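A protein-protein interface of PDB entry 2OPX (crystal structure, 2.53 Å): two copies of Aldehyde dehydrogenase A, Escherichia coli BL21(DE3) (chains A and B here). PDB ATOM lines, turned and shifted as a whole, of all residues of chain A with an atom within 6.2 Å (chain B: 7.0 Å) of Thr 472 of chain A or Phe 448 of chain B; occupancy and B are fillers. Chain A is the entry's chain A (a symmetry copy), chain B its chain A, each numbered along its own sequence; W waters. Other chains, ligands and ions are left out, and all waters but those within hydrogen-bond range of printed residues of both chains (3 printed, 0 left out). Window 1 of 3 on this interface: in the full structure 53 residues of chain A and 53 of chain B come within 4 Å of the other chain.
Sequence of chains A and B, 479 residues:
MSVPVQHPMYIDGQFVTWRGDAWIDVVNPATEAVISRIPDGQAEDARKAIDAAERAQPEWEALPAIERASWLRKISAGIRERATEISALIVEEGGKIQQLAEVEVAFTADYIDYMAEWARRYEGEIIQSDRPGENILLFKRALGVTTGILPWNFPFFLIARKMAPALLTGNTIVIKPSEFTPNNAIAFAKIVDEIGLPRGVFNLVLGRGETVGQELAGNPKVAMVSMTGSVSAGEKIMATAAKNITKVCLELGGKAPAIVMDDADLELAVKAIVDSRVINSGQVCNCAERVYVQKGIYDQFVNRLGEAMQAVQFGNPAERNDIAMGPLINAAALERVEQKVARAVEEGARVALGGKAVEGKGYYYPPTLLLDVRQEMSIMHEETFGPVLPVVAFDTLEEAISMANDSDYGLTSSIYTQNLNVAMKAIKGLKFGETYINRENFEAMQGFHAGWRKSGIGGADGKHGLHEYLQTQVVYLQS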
ATOM      1  N   ILE A 127     -10.329  10.289  13.359  1.00  0.00           N
ATOM      2  CA  ILE A 127      -8.989  10.463  12.811  1.00  0.00           C
ATOM      3  C   ILE A 127      -8.085   9.261  13.070  1.00  0.00           C
ATOM      4  O   ILE A 127      -8.056   8.727  14.180  1.00  0.00           O
ATOM      5  CB  ILE A 127      -8.329  11.721  13.434  1.00  0.00           C
ATOM      6  CG1 ILE A 127      -9.175  12.955  13.121  1.00  0.00           C
ATOM      7  CG2 ILE A 127      -6.921  11.891  12.918  1.00  0.00           C
ATOM      8  CD1 ILE A 127      -8.787  14.187  13.915  1.00  0.00           C
ATOM      9  N   LEU A 138     -13.028  13.067  17.125  1.00  0.00           N
ATOM     10  CA  LEU A 138     -13.144  14.509  17.251  1.00  0.00           C
ATOM     11  C   LEU A 138     -14.619  14.876  17.199  1.00  0.00           C
ATOM     12  O   LEU A 138     -15.259  14.789  16.152  1.00  0.00           O
ATOM     13  CB  LEU A 138     -12.371  15.192  16.126  1.00  0.00           C
ATOM     14  CG  LEU A 138     -12.350  16.718  16.142  1.00  0.00           C
ATOM     15  CD1 LEU A 138     -11.141  17.208  15.358  1.00  0.00           C
ATOM     16  CD2 LEU A 138     -13.650  17.264  15.562  1.00  0.00           C
ATOM     17  N   PHE A 139     -15.159  15.275  18.343  1.00  0.00           N
ATOM     18  CA  PHE A 139     -16.567  15.641  18.437  1.00  0.00           C
ATOM     19  C   PHE A 139     -16.759  17.135  18.253  1.00  0.00           C
ATOM     20  O   PHE A 139     -15.847  17.926  18.499  1.00  0.00           O
ATOM     21  CB  PHE A 139     -17.119  15.261  19.813  1.00  0.00           C
ATOM     22  CG  PHE A 139     -17.216  13.793  20.042  1.00  0.00           C
ATOM     23  CD1 PHE A 139     -18.348  13.092  19.653  1.00  0.00           C
ATOM     24  CD2 PHE A 139     -16.170  13.102  20.648  1.00  0.00           C
ATOM     25  CE1 PHE A 139     -18.441  11.724  19.865  1.00  0.00           C
ATOM     26  CE2 PHE A 139     -16.250  11.733  20.865  1.00  0.00           C
ATOM     27  CZ  PHE A 139     -17.386  11.041  20.475  1.00  0.00           C
ATOM     28  N   LYS A 140     -17.956  17.511  17.821  1.00  0.00           N
ATOM     29  CA  LYS A 140     -18.306  18.911  17.653  1.00  0.00           C
ATOM     30  C   LYS A 140     -19.257  19.182  18.809  1.00  0.00           C
ATOM     31  O   LYS A 140     -20.274  18.496  18.967  1.00  0.00           O
ATOM     32  CB  LYS A 140     -19.021  19.144  16.320  1.00  0.00           C
ATOM     33  CG  LYS A 140     -18.142  19.000  15.086  1.00  0.00           C
ATOM     34  CD  LYS A 140     -17.136  20.129  14.986  1.00  0.00           C
ATOM     35  CE  LYS A 140     -16.370  20.060  13.674  1.00  0.00           C
ATOM     36  NZ  LYS A 140     -15.548  21.289  13.450  1.00  0.00           N
ATOM     37  N   ARG A 141     -18.919  20.169  19.627  1.00  0.00           N
ATOM     38  CA  ARG A 141     -19.743  20.507  20.778  1.00  0.00           C
ATOM     39  C   ARG A 141     -20.155  21.965  20.716  1.00  0.00           C
ATOM     40  O   ARG A 141     -19.574  22.755  19.967  1.00  0.00           O
ATOM     41  CB  ARG A 141     -18.957  20.278  22.073  1.00  0.00           C
ATOM     42  CG  ARG A 141     -18.329  18.905  22.214  1.00  0.00           C
ATOM     43  CD  ARG A 141     -19.366  17.805  22.193  1.00  0.00           C
ATOM     44  NE  ARG A 141     -18.812  16.561  22.713  1.00  0.00           N
ATOM     45  CZ  ARG A 141     -19.455  15.398  22.730  1.00  0.00           C
ATOM     46  NH1 ARG A 141     -20.693  15.305  22.251  1.00  0.00           N
ATOM     47  NH2 ARG A 141     -18.852  14.321  23.214  1.00  0.00           N
ATOM     48  N   LEU A 470     -19.796  25.997  16.908  1.00  0.00           N
ATOM     49  CA  LEU A 470     -19.366  24.661  17.284  1.00  0.00           C
ATOM     50  C   LEU A 470     -17.878  24.667  17.593  1.00  0.00           C
ATOM     51  O   LEU A 470     -17.111  25.397  16.971  1.00  0.00           O
ATOM     52  CB  LEU A 470     -19.641  23.700  16.127  1.00  0.00           C
ATOM     53  CG  LEU A 470     -20.628  22.532  16.228  1.00  0.00           C
ATOM     54  CD1 LEU A 470     -21.671  22.756  17.292  1.00  0.00           C
ATOM     55  CD2 LEU A 470     -21.277  22.350  14.858  1.00  0.00           C
ATOM     56  N   GLN A 471     -17.472  23.869  18.571  1.00  0.00           N
ATOM     57  CA  GLN A 471     -16.062  23.772  18.904  1.00  0.00           C
ATOM     58  C   GLN A 471     -15.742  22.294  18.969  1.00  0.00           C
ATOM     59  O   GLN A 471     -16.643  21.453  18.910  1.00  0.00           O
ATOM     60  CB  GLN A 471     -15.740  24.473  20.226  1.00  0.00           C
ATOM     61  CG  GLN A 471     -16.365  23.874  21.463  1.00  0.00           C
ATOM     62  CD  GLN A 471     -16.107  24.730  22.678  1.00  0.00           C
ATOM     63  OE1 GLN A 471     -15.008  25.266  22.844  1.00  0.00           O
ATOM     64  NE2 GLN A 471     -17.110  24.863  23.539  1.00  0.00           N
ATOM     65  N   THR A 472     -14.465  21.968  19.096  1.00  0.00           N
ATOM     66  CA  THR A 472     -14.078  20.572  19.093  1.00  0.00           C
ATOM     67  C   THR A 472     -13.564  19.954  20.387  1.00  0.00           C
ATOM     68  O   THR A 472     -12.992  20.619  21.251  1.00  0.00           O
ATOM     69  CB  THR A 472     -13.032  20.327  17.991  1.00  0.00           C
ATOM     70  OG1 THR A 472     -11.889  21.151  18.236  1.00  0.00           O
ATOM     71  CG2 THR A 472     -13.608  20.679  16.625  1.00  0.00           C
ATOM     72  N   GLN A 473     -13.800  18.655  20.496  1.00  0.00           N
ATOM     73  CA  GLN A 473     -13.353  17.853  21.620  1.00  0.00           C
ATOM     74  C   GLN A 473     -12.717  16.621  20.997  1.00  0.00           C
ATOM     75  O   GLN A 473     -13.408  15.740  20.485  1.00  0.00           O
ATOM     76  CB  GLN A 473     -14.523  17.433  22.512  1.00  0.00           C
ATOM     77  CG  GLN A 473     -14.166  16.290  23.457  1.00  0.00           C
ATOM     78  CD  GLN A 473     -15.336  15.836  24.301  1.00  0.00           C
ATOM     79  OE1 GLN A 473     -16.462  15.732  23.812  1.00  0.00           O
ATOM     80  NE2 GLN A 473     -15.075  15.544  25.574  1.00  0.00           N
ATOM     81  N   VAL A 474     -11.393  16.584  21.010  1.00  0.00           N
ATOM     82  CA  VAL A 474     -10.668  15.457  20.454  1.00  0.00           C
ATOM     83  C   VAL A 474     -10.485  14.408  21.543  1.00  0.00           C
ATOM     84  O   VAL A 474      -9.844  14.661  22.563  1.00  0.00           O
ATOM     85  CB  VAL A 474      -9.291  15.896  19.923  1.00  0.00           C
ATOM     86  CG1 VAL A 474      -8.510  14.689  19.422  1.00  0.00           C
ATOM     87  CG2 VAL A 474      -9.482  16.916  18.811  1.00  0.00           C
ATOM     88  N   TYR A 476      -8.961  10.844  22.661  1.00  0.00           N
ATOM     89  CA  TYR A 476      -7.965   9.826  22.355  1.00  0.00           C
ATOM     90  C   TYR A 476      -8.341   8.596  23.174  1.00  0.00           C
ATOM     91  O   TYR A 476      -7.974   8.481  24.339  1.00  0.00           O
ATOM     92  CB  TYR A 476      -6.563  10.287  22.744  1.00  0.00           C
ATOM     93  CG  TYR A 476      -6.019  11.408  21.900  1.00  0.00           C
ATOM     94  CD1 TYR A 476      -6.369  12.731  22.157  1.00  0.00           C
ATOM     95  CD2 TYR A 476      -5.136  11.147  20.849  1.00  0.00           C
ATOM     96  CE1 TYR A 476      -5.850  13.773  21.393  1.00  0.00           C
ATOM     97  CE2 TYR A 476      -4.614  12.179  20.076  1.00  0.00           C
ATOM     98  CZ  TYR A 476      -4.975  13.491  20.357  1.00  0.00           C
ATOM     99  OH  TYR A 476      -4.455  14.520  19.612  1.00  0.00           O
ATOM    100  N   ARG B 161       4.901  24.572  14.802  1.00  0.00           N
ATOM    101  CA  ARG B 161       3.470  24.485  15.042  1.00  0.00           C
ATOM    102  C   ARG B 161       2.748  25.664  14.409  1.00  0.00           C
ATOM    103  O   ARG B 161       1.606  25.536  13.955  1.00  0.00           O
ATOM    104  CB  ARG B 161       3.183  24.424  16.546  1.00  0.00           C
ATOM    105  CG  ARG B 161       1.721  24.228  16.885  1.00  0.00           C
ATOM    106  CD  ARG B 161       1.528  23.927  18.353  1.00  0.00           C
ATOM    107  NE  ARG B 161       0.983  22.590  18.555  1.00  0.00           N
ATOM    108  CZ  ARG B 161       0.702  22.059  19.741  1.00  0.00           C
ATOM    109  NH1 ARG B 161       0.914  22.749  20.854  1.00  0.00           N
ATOM    110  NH2 ARG B 161       0.202  20.837  19.811  1.00  0.00           N
ATOM    111  N   GLY B 410      -9.827  24.741  29.759  1.00  0.00           N
ATOM    112  CA  GLY B 410     -10.517  23.591  29.214  1.00  0.00           C
ATOM    113  C   GLY B 410      -9.760  23.022  28.033  1.00  0.00           C
ATOM    114  O   GLY B 410     -10.349  22.670  27.005  1.00  0.00           O
ATOM    115  N   LEU B 411      -8.444  22.928  28.185  1.00  0.00           N
ATOM    116  CA  LEU B 411      -7.594  22.411  27.121  1.00  0.00           C
ATOM    117  C   LEU B 411      -7.562  20.896  27.076  1.00  0.00           C
ATOM    118  O   LEU B 411      -7.952  20.282  26.082  1.00  0.00           O
ATOM    119  CB  LEU B 411      -6.160  22.930  27.282  1.00  0.00           C
ATOM    120  CG  LEU B 411      -5.135  22.378  26.285  1.00  0.00           C
ATOM    121  CD1 LEU B 411      -5.510  22.809  24.868  1.00  0.00           C
ATOM    122  CD2 LEU B 411      -3.743  22.876  26.644  1.00  0.00           C
ATOM    123  N   PHE B 432     -13.993  19.828  27.405  1.00  0.00           N
ATOM    124  CA  PHE B 432     -12.594  20.090  27.094  1.00  0.00           C
ATOM    125  C   PHE B 432     -12.298  19.896  25.616  1.00  0.00           C
ATOM    126  O   PHE B 432     -13.057  19.238  24.903  1.00  0.00           O
ATOM    127  CB  PHE B 432     -11.684  19.170  27.926  1.00  0.00           C
ATOM    128  CG  PHE B 432     -11.598  19.557  29.375  1.00  0.00           C
ATOM    129  CD1 PHE B 432     -12.662  19.304  30.244  1.00  0.00           C
ATOM    130  CD2 PHE B 432     -10.487  20.250  29.853  1.00  0.00           C
ATOM    131  CE1 PHE B 432     -12.624  19.746  31.565  1.00  0.00           C
ATOM    132  CE2 PHE B 432     -10.440  20.698  31.174  1.00  0.00           C
ATOM    133  CZ  PHE B 432     -11.510  20.448  32.032  1.00  0.00           C
ATOM    134  N   GLY B 433     -11.194  20.473  25.158  1.00  0.00           N
ATOM    135  CA  GLY B 433     -10.829  20.332  23.762  1.00  0.00           C
ATOM    136  C   GLY B 433     -10.182  18.985  23.532  1.00  0.00           C
ATOM    137  O   GLY B 433     -10.102  18.497  22.404  1.00  0.00           O
ATOM    138  N   GLU B 434      -9.718  18.383  24.622  1.00  0.00           N
ATOM    139  CA  GLU B 434      -9.070  17.081  24.570  1.00  0.00           C
ATOM    140  C   GLU B 434      -9.395  16.227  25.789  1.00  0.00           C
ATOM    141  O   GLU B 434      -9.424  16.706  26.926  1.00  0.00           O
ATOM    142  CB  GLU B 434      -7.553  17.233  24.493  1.00  0.00           C
ATOM    143  CG  GLU B 434      -7.018  17.722  23.174  1.00  0.00           C
ATOM    144  CD  GLU B 434      -5.540  18.066  23.258  1.00  0.00           C
ATOM    145  OE1 GLU B 434      -4.932  18.349  22.202  1.00  0.00           O
ATOM    146  OE2 GLU B 434      -4.992  18.059  24.385  1.00  0.00           O
ATOM    147  N   GLU B 443      -0.696  15.073  22.571  1.00  0.00           N
ATOM    148  CA  GLU B 443      -1.434  15.285  21.329  1.00  0.00           C
ATOM    149  C   GLU B 443      -0.721  14.706  20.118  1.00  0.00           C
ATOM    150  O   GLU B 443       0.509  14.692  20.058  1.00  0.00           O
ATOM    151  CB  GLU B 443      -1.654  16.769  21.031  1.00  0.00           C
ATOM    152  CG  GLU B 443      -1.875  17.669  22.200  1.00  0.00           C
ATOM    153  CD  GLU B 443      -0.575  18.167  22.769  1.00  0.00           C
ATOM    154  OE1 GLU B 443       0.088  17.385  23.479  1.00  0.00           O
ATOM    155  OE2 GLU B 443      -0.209  19.333  22.495  1.00  0.00           O
ATOM    156  N   ALA B 444      -1.509  14.243  19.154  1.00  0.00           N
ATOM    157  CA  ALA B 444      -0.986  13.703  17.904  1.00  0.00           C
ATOM    158  C   ALA B 444      -0.923  14.899  16.965  1.00  0.00           C
ATOM    159  O   ALA B 444      -1.706  15.842  17.107  1.00  0.00           O
ATOM    160  CB  ALA B 444      -1.931  12.652  17.341  1.00  0.00           C
ATOM    161  N   MET B 445      -0.003  14.879  16.008  1.00  0.00           N
ATOM    162  CA  MET B 445       0.100  16.001  15.083  1.00  0.00           C
ATOM    163  C   MET B 445      -1.149  16.120  14.207  1.00  0.00           C
ATOM    164  O   MET B 445      -1.434  17.188  13.666  1.00  0.00           O
ATOM    165  CB  MET B 445       1.350  15.865  14.205  1.00  0.00           C
ATOM    166  CG  MET B 445       1.432  14.579  13.405  1.00  0.00           C
ATOM    167  SD  MET B 445       2.914  14.522  12.373  1.00  0.00           S
ATOM    168  CE  MET B 445       4.171  14.129  13.582  1.00  0.00           C
ATOM    169  N   GLN B 446      -1.894  15.028  14.079  1.00  0.00           N
ATOM    170  CA  GLN B 446      -3.097  15.028  13.267  1.00  0.00           C
ATOM    171  C   GLN B 446      -4.357  15.235  14.095  1.00  0.00           C
ATOM    172  O   GLN B 446      -5.466  15.010  13.609  1.00  0.00           O
ATOM    173  CB  GLN B 446      -3.220  13.724  12.478  1.00  0.00           C
ATOM    174  CG  GLN B 446      -3.477  12.477  13.321  1.00  0.00           C
ATOM    175  CD  GLN B 446      -2.206  11.730  13.693  1.00  0.00           C
ATOM    176  OE1 GLN B 446      -2.164  10.498  13.643  1.00  0.00           O
ATOM    177  NE2 GLN B 446      -1.169  12.467  14.073  1.00  0.00           N
ATOM    178  N   GLY B 447      -4.190  15.647  15.347  1.00  0.00           N
ATOM    179  CA  GLY B 447      -5.344  15.893  16.188  1.00  0.00           C
ATOM    180  C   GLY B 447      -5.626  17.382  16.142  1.00  0.00           C
ATOM    181  O   GLY B 447      -5.176  18.063  15.222  1.00  0.00           O
ATOM    182  N   PHE B 448      -6.368  17.896  17.116  1.00  0.00           N
ATOM    183  CA  PHE B 448      -6.654  19.320  17.150  1.00  0.00           C
ATOM    184  C   PHE B 448      -6.493  19.850  18.565  1.00  0.00           C
ATOM    185  O   PHE B 448      -7.380  19.715  19.407  1.00  0.00           O
ATOM    186  CB  PHE B 448      -8.063  19.607  16.631  1.00  0.00           C
ATOM    187  CG  PHE B 448      -8.328  21.069  16.393  1.00  0.00           C
ATOM    188  CD1 PHE B 448      -7.332  21.893  15.861  1.00  0.00           C
ATOM    189  CD2 PHE B 448      -9.571  21.624  16.683  1.00  0.00           C
ATOM    190  CE1 PHE B 448      -7.568  23.244  15.621  1.00  0.00           C
ATOM    191  CE2 PHE B 448      -9.819  22.979  16.448  1.00  0.00           C
ATOM    192  CZ  PHE B 448      -8.814  23.790  15.915  1.00  0.00           C
ATOM    193  N   HIS B 449      -5.335  20.444  18.818  1.00  0.00           N
ATOM    194  CA  HIS B 449      -5.004  20.995  20.123  1.00  0.00           C
ATOM    195  C   HIS B 449      -5.605  22.392  20.233  1.00  0.00           C
ATOM    196  O   HIS B 449      -4.932  23.391  19.984  1.00  0.00           O
ATOM    197  CB  HIS B 449      -3.486  21.053  20.259  1.00  0.00           C
ATOM    198  CG  HIS B 449      -3.004  21.314  21.651  1.00  0.00           C
ATOM    199  ND1 HIS B 449      -3.190  20.420  22.683  1.00  0.00           N
ATOM    200  CD2 HIS B 449      -2.306  22.352  22.172  1.00  0.00           C
ATOM    201  CE1 HIS B 449      -2.628  20.896  23.780  1.00  0.00           C
ATOM    202  NE2 HIS B 449      -2.085  22.067  23.496  1.00  0.00           N
ATOM    203  N   ALA B 450      -6.880  22.453  20.603  1.00  0.00           N
ATOM    204  CA  ALA B 450      -7.591  23.718  20.742  1.00  0.00           C
ATOM    205  C   ALA B 450      -8.334  23.730  22.078  1.00  0.00           C
ATOM    206  O   ALA B 450      -9.272  22.962  22.283  1.00  0.00           O
ATOM    207  CB  ALA B 450      -8.563  23.885  19.582  1.00  0.00           C
ATOM    208  N   GLY B 451      -7.916  24.613  22.980  1.00  0.00           N
ATOM    209  CA  GLY B 451      -8.522  24.675  24.297  1.00  0.00           C
ATOM    210  C   GLY B 451      -9.787  25.488  24.448  1.00  0.00           C
ATOM    211  O   GLY B 451      -9.957  26.538  23.825  1.00  0.00           O
ATOM    212  N   TRP B 452     -10.685  24.987  25.290  1.00  0.00           N
ATOM    213  CA  TRP B 452     -11.943  25.665  25.570  1.00  0.00           C
ATOM    214  C   TRP B 452     -11.723  26.784  26.575  1.00  0.00           C
ATOM    215  O   TRP B 452     -10.650  26.903  27.182  1.00  0.00           O
ATOM    216  CB  TRP B 452     -12.961  24.693  26.155  1.00  0.00           C
ATOM    217  CG  TRP B 452     -13.434  23.668  25.192  1.00  0.00           C
ATOM    218  CD1 TRP B 452     -12.733  23.135  24.152  1.00  0.00           C
ATOM    219  CD2 TRP B 452     -14.694  22.995  25.216  1.00  0.00           C
ATOM    220  NE1 TRP B 452     -13.476  22.168  23.530  1.00  0.00           N
ATOM    221  CE2 TRP B 452     -14.685  22.058  24.162  1.00  0.00           C
ATOM    222  CE3 TRP B 452     -15.830  23.091  26.026  1.00  0.00           C
ATOM    223  CZ2 TRP B 452     -15.770  21.219  23.895  1.00  0.00           C
ATOM    224  CZ3 TRP B 452     -16.912  22.257  25.758  1.00  0.00           C
ATOM    225  CH2 TRP B 452     -16.871  21.334  24.703  1.00  0.00           C
ATOM    226  N   GLY B 458      -9.165  29.313  18.903  1.00  0.00           N
ATOM    227  CA  GLY B 458      -8.592  28.661  17.741  1.00  0.00           C
ATOM    228  C   GLY B 458      -7.812  27.455  18.237  1.00  0.00           C
ATOM    229  O   GLY B 458      -7.998  27.022  19.376  1.00  0.00           O
ATOM    230  N   GLY B 459      -6.938  26.907  17.402  1.00  0.00           N
ATOM    231  CA  GLY B 459      -6.169  25.754  17.827  1.00  0.00           C
ATOM    232  C   GLY B 459      -4.959  25.488  16.962  1.00  0.00           C
ATOM    233  O   GLY B 459      -4.643  26.272  16.071  1.00  0.00           O
ATOM    234  N   ALA B 460      -4.289  24.372  17.221  1.00  0.00           N
ATOM    235  CA  ALA B 460      -3.101  23.996  16.470  1.00  0.00           C
ATOM    236  C   ALA B 460      -3.150  22.522  16.105  1.00  0.00           C
ATOM    237  O   ALA B 460      -3.895  21.751  16.707  1.00  0.00           O
ATOM    238  CB  ALA B 460      -1.865  24.267  17.299  1.00  0.00           C
ATOM    239  N   ASP B 461      -2.352  22.146  15.109  1.00  0.00           N
ATOM    240  CA  ASP B 461      -2.245  20.761  14.654  1.00  0.00           C
ATOM    241  C   ASP B 461      -3.389  20.309  13.765  1.00  0.00           C
ATOM    242  O   ASP B 461      -4.449  20.927  13.724  1.00  0.00           O
ATOM    243  CB  ASP B 461      -2.156  19.814  15.857  1.00  0.00           C
ATOM    244  CG  ASP B 461      -1.137  20.261  16.882  1.00  0.00           C
ATOM    245  OD1 ASP B 461      -1.181  19.743  18.017  1.00  0.00           O
ATOM    246  OD2 ASP B 461      -0.290  21.125  16.560  1.00  0.00           O
ATOM    247  N   GLY B 462      -3.150  19.214  13.057  1.00  0.00           N
ATOM    248  CA  GLY B 462      -4.150  18.633  12.186  1.00  0.00           C
ATOM    249  C   GLY B 462      -4.742  19.531  11.120  1.00  0.00           C
ATOM    250  O   GLY B 462      -4.221  20.605  10.822  1.00  0.00           O
ATOM    251  N   LYS B 463      -5.847  19.063  10.547  1.00  0.00           N
ATOM    252  CA  LYS B 463      -6.560  19.773   9.500  1.00  0.00           C
ATOM    253  C   LYS B 463      -7.105  21.106   9.993  1.00  0.00           C
ATOM    254  O   LYS B 463      -7.025  22.122   9.299  1.00  0.00           O
ATOM    255  CB  LYS B 463      -7.714  18.907   8.993  1.00  0.00           C
ATOM    256  CG  LYS B 463      -8.555  19.554   7.914  1.00  0.00           C
ATOM    257  CD  LYS B 463      -9.701  18.645   7.504  1.00  0.00           C
ATOM    258  CE  LYS B 463     -10.652  18.412   8.669  1.00  0.00           C
ATOM    259  NZ  LYS B 463     -11.853  17.638   8.260  1.00  0.00           N
ATOM    260  N   HIS B 464      -7.652  21.098  11.201  1.00  0.00           N
ATOM    261  CA  HIS B 464      -8.228  22.303  11.760  1.00  0.00           C
ATOM    262  C   HIS B 464      -7.176  23.310  12.164  1.00  0.00           C
ATOM    263  O   HIS B 464      -7.443  24.511  12.189  1.00  0.00           O
ATOM    264  CB  HIS B 464      -9.139  21.942  12.929  1.00  0.00           C
ATOM    265  CG  HIS B 464     -10.256  21.031  12.536  1.00  0.00           C
ATOM    266  ND1 HIS B 464     -10.159  19.659  12.618  1.00  0.00           N
ATOM    267  CD2 HIS B 464     -11.450  21.289  11.953  1.00  0.00           C
ATOM    268  CE1 HIS B 464     -11.243  19.110  12.100  1.00  0.00           C
ATOM    269  NE2 HIS B 464     -12.042  20.077  11.689  1.00  0.00           N
ATOM    270  N   GLY B 465      -5.979  22.824  12.476  1.00  0.00           N
ATOM    271  CA  GLY B 465      -4.902  23.727  12.837  1.00  0.00           C
ATOM    272  C   GLY B 465      -4.502  24.443  11.563  1.00  0.00           C
ATOM    273  O   GLY B 465      -4.303  25.661  11.540  1.00  0.00           O
ATOM    274  N   LEU B 466      -4.406  23.652  10.498  1.00  0.00           N
ATOM    275  CA  LEU B 466      -4.062  24.119   9.163  1.00  0.00           C
ATOM    276  C   LEU B 466      -5.074  25.176   8.699  1.00  0.00           C
ATOM    277  O   LEU B 466      -4.692  26.231   8.197  1.00  0.00           O
ATOM    278  CB  LEU B 466      -4.063  22.914   8.214  1.00  0.00           C
ATOM    279  CG  LEU B 466      -3.550  22.925   6.767  1.00  0.00           C
ATOM    280  CD1 LEU B 466      -4.649  23.330   5.821  1.00  0.00           C
ATOM    281  CD2 LEU B 466      -2.327  23.820   6.653  1.00  0.00           C
ATOM    282  N   GLU B 468      -6.665  27.197  10.343  1.00  0.00           N
ATOM    283  CA  GLU B 468      -6.600  28.416  11.144  1.00  0.00           C
ATOM    284  C   GLU B 468      -5.904  29.483  10.299  1.00  0.00           C
ATOM    285  O   GLU B 468      -6.114  30.682  10.480  1.00  0.00           O
ATOM    286  CB  GLU B 468      -5.774  28.195  12.410  1.00  0.00           C
ATOM    287  CG  GLU B 468      -6.497  27.540  13.569  1.00  0.00           C
ATOM    288  CD  GLU B 468      -7.664  28.364  14.064  1.00  0.00           C
ATOM    289  OE1 GLU B 468      -7.622  29.608  13.927  1.00  0.00           O
ATOM    290  OE2 GLU B 468      -8.620  27.763  14.601  1.00  0.00           O
HETATM  291  O   HOH W   1      -9.855  20.170  20.124  1.00  0.00           O
HETATM  292  O   HOH W   2      -5.154  17.151  19.659  1.00  0.00           O
HETATM  293  O   HOH W   3     -11.718  23.124  21.153  1.00  0.00           O
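O of Gly 433 of chain B lies within hydrogen-bond range of N of Val 474 of chain A (2.7 Å). The side-chain hydroxyl (OH) of Tyr 476 of chain A lies within hydrogen-bond range of the backbone NH (N) of Ala 444 of chain B. NE1 of Trp 452 of chain B is in hydrogen-bond range of O of Thr 472 of chain A (2.8 Å).
O of Gly 410 of chain B is in hydrogen-bond range of N of Gly 433 of chain B (3.0 Å). O of Leu 411 of chain B is in hydrogen-bond range of N of Gly 433 of chain B (3.4 Å). The backbone NH (N) of Glu 434 of chain B lies within hydrogen-bond range of the backbone carbonyl oxygen (O) of Leu 411 of chain B. The backbone NH (N) of Gly 462 of chain B is in hydrogen-bond range of the backbone carbonyl oxygen (O) of Gly 447 of chain B, at 3.2 Å. The backbone carbonyl oxygen (O) of Gln 471 of chain A is in hydrogen-bond range of the backbone NH (N) of Arg 141 of chain A, 2.7 Å away.
Gln 446 of chain B touches Ile 127 of chain A (O to CD1, 3.4 Å). His 464 of chain B touches Leu 138 of chain A. CB of Arg 141 of chain A touches CH2 of Trp 452 of chain B (3.5 Å). Trp 452 of chain B touches Gln 471 of chain A. O of Thr 472 of chain A touches O of Phe 432 of chain B (3.9 Å). Gly 433 of chain B touches Thr 472 of chain A. Thr 472 of chain A touches Phe 448 of chain B. Gln 473 of chain A touches Gly 433 of chain B. Val 474 of chain A touches Phe 448 of chain B (CG2 to O, 3.6 Å). OH of Tyr 476 of chain A touches CA of Glu 443 of chain B, 3.6 Å away.
Lys 140 of chain A touches none of the printed residues of chain B. Thr 472 of chain A touches just these residues of chain B: Phe 432 (3.9 Å), Gly 433 (3.3 Å), Phe 448 (2.8 Å) and Trp 452 (2.8 Å). Of the printed residues of chain B, Val 474 of chain A touches Gly 433, Glu 434 and Phe 448. Of the printed residues of chain A, Glu 443 of chain B touches Tyr 476 (3.6 Å). Printed residues of chain A within 4 Å of Gly 447 of chain B: Tyr 476 (3.8 Å). Phe 448 of chain B touches two residues of chain A. Of the printed residues of chain A, His 464 of chain B touches Leu 138 (3.8 Å).
Of the 26 printed residues of chain B, 10 touch a printed residue of chain A. Printed residues of chain B that touch a printed residue of chain A: Phe 432, Gly 433, Glu 434, Glu 443, Ala 444, Gln 446, Gly 447, Phe 448, Trp 452 and His 464. Hydrophobic or aromatic side chains of chain B within 4 Å of the printed part of chain A: Ala 444, Phe 448, Trp 452 and His 464. Of the 11 printed residues of chain A, 8 touch a printed residue of chain B. Among the printed residues, 16 pairs touch across the chains.
No position is printed for both chains.
Water W1 lies within hydrogen-bond range of the backbone carbonyl oxygen of Phe 448 of chain B (2.6 Å), the backbone carbonyl oxygen of Gly 433 of chain B (2.8 Å) and the side-chain hydroxyl of Thr 472 of chain A (2.9 Å). Water W3 lies within hydrogen-bond range of O of Ala 450 of chain B (2.7 Å), O of Thr 472 of chain A (2.8 Å) and NE1 of Trp 452 of chain B (3.1 Å). Water W2 lies within hydrogen-bond range of the side-chain hydroxyl of Tyr 476 of chain A (2.7 Å), the side-chain carboxylate of Glu 434 of chain B (2.8 Å), the backbone NH of Phe 448 of chain B (2.9 Å) and the backbone NH of His 449 of chain B (3.4 Å).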
